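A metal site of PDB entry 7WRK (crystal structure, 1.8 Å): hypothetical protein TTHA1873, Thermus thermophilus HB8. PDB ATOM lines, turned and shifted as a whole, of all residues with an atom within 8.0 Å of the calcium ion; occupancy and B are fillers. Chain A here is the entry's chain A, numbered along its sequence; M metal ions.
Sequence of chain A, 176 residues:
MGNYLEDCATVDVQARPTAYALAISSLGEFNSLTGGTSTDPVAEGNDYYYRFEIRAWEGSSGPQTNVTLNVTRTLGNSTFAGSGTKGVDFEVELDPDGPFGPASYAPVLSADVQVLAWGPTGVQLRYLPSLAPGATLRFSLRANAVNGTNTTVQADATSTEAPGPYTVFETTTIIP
The calcium ion is bound by the side-chain carboxylate (OD1) of Asp 97 (2.2 Å), the backbone carbonyl oxygen (O) of Ala 103 (2.3 Å), the backbone carbonyl oxygen (O) of Gly 98 (2.4 Å), the side-chain carboxylate (OD1) of Asp 95 (2.4 Å), the backbone carbonyl oxygen (O) of Gly 101 (2.5 Å) and the side-chain carboxylate (OD2) of Asp 95 (2.5 Å).
Of the 15 residues printed, 5 come within 4 Å of the calcium ion.
The nearest printed residue that does not touch the calcium ion is Pro 102 (4.005 Å).
The backbone NH (N) of Asp 95 lies within hydrogen-bond range of the backbone carbonyl oxygen (O) of Thr 136 (2.9 Å).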
ATOM      1  N   LEU A  94       3.606  15.386 -18.592  1.00  0.00           N
ATOM      2  CA  LEU A  94       3.210  14.429 -17.557  1.00  0.00           C
ATOM      3  C   LEU A  94       2.851  13.077 -18.174  1.00  0.00           C
ATOM      4  O   LEU A  94       2.154  13.085 -19.164  1.00  0.00           O
ATOM      5  CB  LEU A  94       2.005  14.953 -16.772  1.00  0.00           C
ATOM      6  CG  LEU A  94       1.386  14.000 -15.734  1.00  0.00           C
ATOM      7  CD1 LEU A  94       2.313  13.764 -14.538  1.00  0.00           C
ATOM      8  CD2 LEU A  94       0.056  14.521 -15.202  1.00  0.00           C
ATOM      9  N   ASP A  95       3.342  11.998 -17.554  1.00  0.00           N
ATOM     10  CA  ASP A  95       2.938  10.622 -17.898  1.00  0.00           C
ATOM     11  C   ASP A  95       2.220  10.186 -16.646  1.00  0.00           C
ATOM     12  O   ASP A  95       2.875   9.769 -15.701  1.00  0.00           O
ATOM     13  CB  ASP A  95       4.126   9.677 -18.159  1.00  0.00           C
ATOM     14  CG  ASP A  95       3.623   8.293 -18.513  1.00  0.00           C
ATOM     15  OD1 ASP A  95       2.429   8.019 -18.221  1.00  0.00           O
ATOM     16  OD2 ASP A  95       4.426   7.470 -19.064  1.00  0.00           O
ATOM     17  N   PRO A  96       0.887  10.323 -16.616  1.00  0.00           N
ATOM     18  CA  PRO A  96       0.150  10.164 -15.356  1.00  0.00           C
ATOM     19  C   PRO A  96       0.234   8.773 -14.735  1.00  0.00           C
ATOM     20  O   PRO A  96      -0.084   8.666 -13.521  1.00  0.00           O
ATOM     21  CB  PRO A  96      -1.272  10.604 -15.737  1.00  0.00           C
ATOM     22  CG  PRO A  96      -1.357  10.365 -17.234  1.00  0.00           C
ATOM     23  CD  PRO A  96       0.036  10.653 -17.769  1.00  0.00           C
ATOM     24  N   ASP A  97       0.506   7.738 -15.541  1.00  0.00           N
ATOM     25  CA  ASP A  97       0.646   6.377 -14.965  1.00  0.00           C
ATOM     26  C   ASP A  97       2.108   5.911 -15.012  1.00  0.00           C
ATOM     27  O   ASP A  97       2.350   4.749 -14.646  1.00  0.00           O
ATOM     28  CB  ASP A  97      -0.342   5.395 -15.594  1.00  0.00           C
ATOM     29  CG  ASP A  97      -0.178   5.301 -17.095  1.00  0.00           C
ATOM     30  OD1 ASP A  97       0.869   5.813 -17.587  1.00  0.00           O
ATOM     31  OD2 ASP A  97      -1.093   4.739 -17.763  1.00  0.00           O
ATOM     32  N   GLY A  98       3.015   6.802 -15.358  1.00  0.00           N
ATOM     33  CA  GLY A  98       4.428   6.455 -15.343  1.00  0.00           C
ATOM     34  C   GLY A  98       4.657   5.233 -16.242  1.00  0.00           C
ATOM     35  O   GLY A  98       3.935   4.962 -17.193  1.00  0.00           O
ATOM     36  N   PRO A  99       5.718   4.467 -15.957  1.00  0.00           N
ATOM     37  CA  PRO A  99       6.011   3.259 -16.698  1.00  0.00           C
ATOM     38  C   PRO A  99       4.988   2.177 -16.420  1.00  0.00           C
ATOM     39  O   PRO A  99       5.023   1.121 -17.038  1.00  0.00           O
ATOM     40  CB  PRO A  99       7.400   2.876 -16.114  1.00  0.00           C
ATOM     41  CG  PRO A  99       7.408   3.398 -14.739  1.00  0.00           C
ATOM     42  CD  PRO A  99       6.635   4.695 -14.834  1.00  0.00           C
ATOM     43  N   PHE A 100       4.091   2.368 -15.443  1.00  0.00           N
ATOM     44  CA  PHE A 100       3.225   1.260 -15.009  1.00  0.00           C
ATOM     45  C   PHE A 100       1.941   1.162 -15.821  1.00  0.00           C
ATOM     46  O   PHE A 100       1.158   0.283 -15.549  1.00  0.00           O
ATOM     47  CB  PHE A 100       2.896   1.414 -13.531  1.00  0.00           C
ATOM     48  CG  PHE A 100       4.127   1.597 -12.687  1.00  0.00           C
ATOM     49  CD1 PHE A 100       4.961   0.525 -12.396  1.00  0.00           C
ATOM     50  CD2 PHE A 100       4.499   2.844 -12.214  1.00  0.00           C
ATOM     51  CE1 PHE A 100       6.121   0.714 -11.657  1.00  0.00           C
ATOM     52  CE2 PHE A 100       5.660   3.019 -11.501  1.00  0.00           C
ATOM     53  CZ  PHE A 100       6.450   1.945 -11.185  1.00  0.00           C
ATOM     54  N   GLY A 101       1.731   2.106 -16.743  1.00  0.00           N
ATOM     55  CA  GLY A 101       0.527   2.109 -17.588  1.00  0.00           C
ATOM     56  C   GLY A 101       0.767   2.735 -18.946  1.00  0.00           C
ATOM     57  O   GLY A 101       1.800   3.394 -19.161  1.00  0.00           O
ATOM     58  N   PRO A 102      -0.206   2.558 -19.847  1.00  0.00           N
ATOM     59  CA  PRO A 102      -0.007   2.944 -21.248  1.00  0.00           C
ATOM     60  C   PRO A 102      -0.160   4.422 -21.600  1.00  0.00           C
ATOM     61  O   PRO A 102       0.079   4.818 -22.704  1.00  0.00           O
ATOM     62  CB  PRO A 102      -1.086   2.141 -21.969  1.00  0.00           C
ATOM     63  CG  PRO A 102      -2.166   1.899 -20.951  1.00  0.00           C
ATOM     64  CD  PRO A 102      -1.438   1.844 -19.622  1.00  0.00           C
ATOM     65  N   ALA A 103      -0.626   5.205 -20.642  1.00  0.00           N
ATOM     66  CA  ALA A 103      -0.770   6.664 -20.904  1.00  0.00           C
ATOM     67  C   ALA A 103       0.576   7.187 -21.367  1.00  0.00           C
ATOM     68  O   ALA A 103       1.631   6.703 -20.912  1.00  0.00           O
ATOM     69  CB  ALA A 103      -1.253   7.399 -19.712  1.00  0.00           C
ATOM     70  N   SER A 104       0.551   8.106 -22.328  1.00  0.00           N
ATOM     71  CA  SER A 104       1.796   8.713 -22.841  1.00  0.00           C
ATOM     72  C   SER A 104       2.044  10.080 -22.214  1.00  0.00           C
ATOM     73  O   SER A 104       1.161  10.671 -21.612  1.00  0.00           O
ATOM     74  CB  SER A 104       1.702   8.808 -24.318  1.00  0.00           C
ATOM     75  OG  SER A 104       1.704   7.533 -24.921  1.00  0.00           O
ATOM     76  N   TYR A 105       3.248  10.556 -22.365  1.00  0.00           N
ATOM     77  CA  TYR A 105       3.588  11.947 -22.005  1.00  0.00           C
ATOM     78  C   TYR A 105       2.697  12.914 -22.799  1.00  0.00           C
ATOM     79  O   TYR A 105       2.495  12.726 -24.010  1.00  0.00           O
ATOM     80  CB  TYR A 105       5.041  12.265 -22.311  1.00  0.00           C
ATOM     81  CG  TYR A 105       5.972  11.868 -21.195  1.00  0.00           C
ATOM     82  CD1 TYR A 105       5.918  12.531 -19.978  1.00  0.00           C
ATOM     83  CD2 TYR A 105       6.861  10.823 -21.334  1.00  0.00           C
ATOM     84  CE1 TYR A 105       6.763  12.166 -18.932  1.00  0.00           C
ATOM     85  CE2 TYR A 105       7.687  10.434 -20.287  1.00  0.00           C
ATOM     86  CZ  TYR A 105       7.652  11.133 -19.089  1.00  0.00           C
ATOM     87  OH  TYR A 105       8.452  10.833 -18.042  1.00  0.00           O
ATOM     88  N   GLY A 134       3.970   6.938  -8.718  1.00  0.00           N
ATOM     89  CA  GLY A 134       4.217   6.217  -9.987  1.00  0.00           C
ATOM     90  C   GLY A 134       4.287   7.132 -11.170  1.00  0.00           C
ATOM     91  O   GLY A 134       4.942   6.778 -12.129  1.00  0.00           O
ATOM     92  N   ALA A 135       3.708   8.322 -11.079  1.00  0.00           N
ATOM     93  CA  ALA A 135       3.673   9.259 -12.229  1.00  0.00           C
ATOM     94  C   ALA A 135       5.064   9.813 -12.491  1.00  0.00           C
ATOM     95  O   ALA A 135       5.876   9.799 -11.564  1.00  0.00           O
ATOM     96  CB  ALA A 135       2.699  10.390 -11.992  1.00  0.00           C
ATOM     97  N   THR A 136       5.314  10.236 -13.712  1.00  0.00           N
ATOM     98  CA  THR A 136       6.612  10.866 -14.095  1.00  0.00           C
ATOM     99  C   THR A 136       6.396  12.170 -14.836  1.00  0.00           C
ATOM    100  O   THR A 136       5.419  12.286 -15.532  1.00  0.00           O
ATOM    101  CB  THR A 136       7.514   9.969 -14.954  1.00  0.00           C
ATOM    102  OG1 THR A 136       6.911   9.697 -16.211  1.00  0.00           O
ATOM    103  CG2 THR A 136       7.722   8.631 -14.274  1.00  0.00           C
HETATM  104 CA    CA M   1       2.592   5.732 -19.002  1.00  0.00          CA
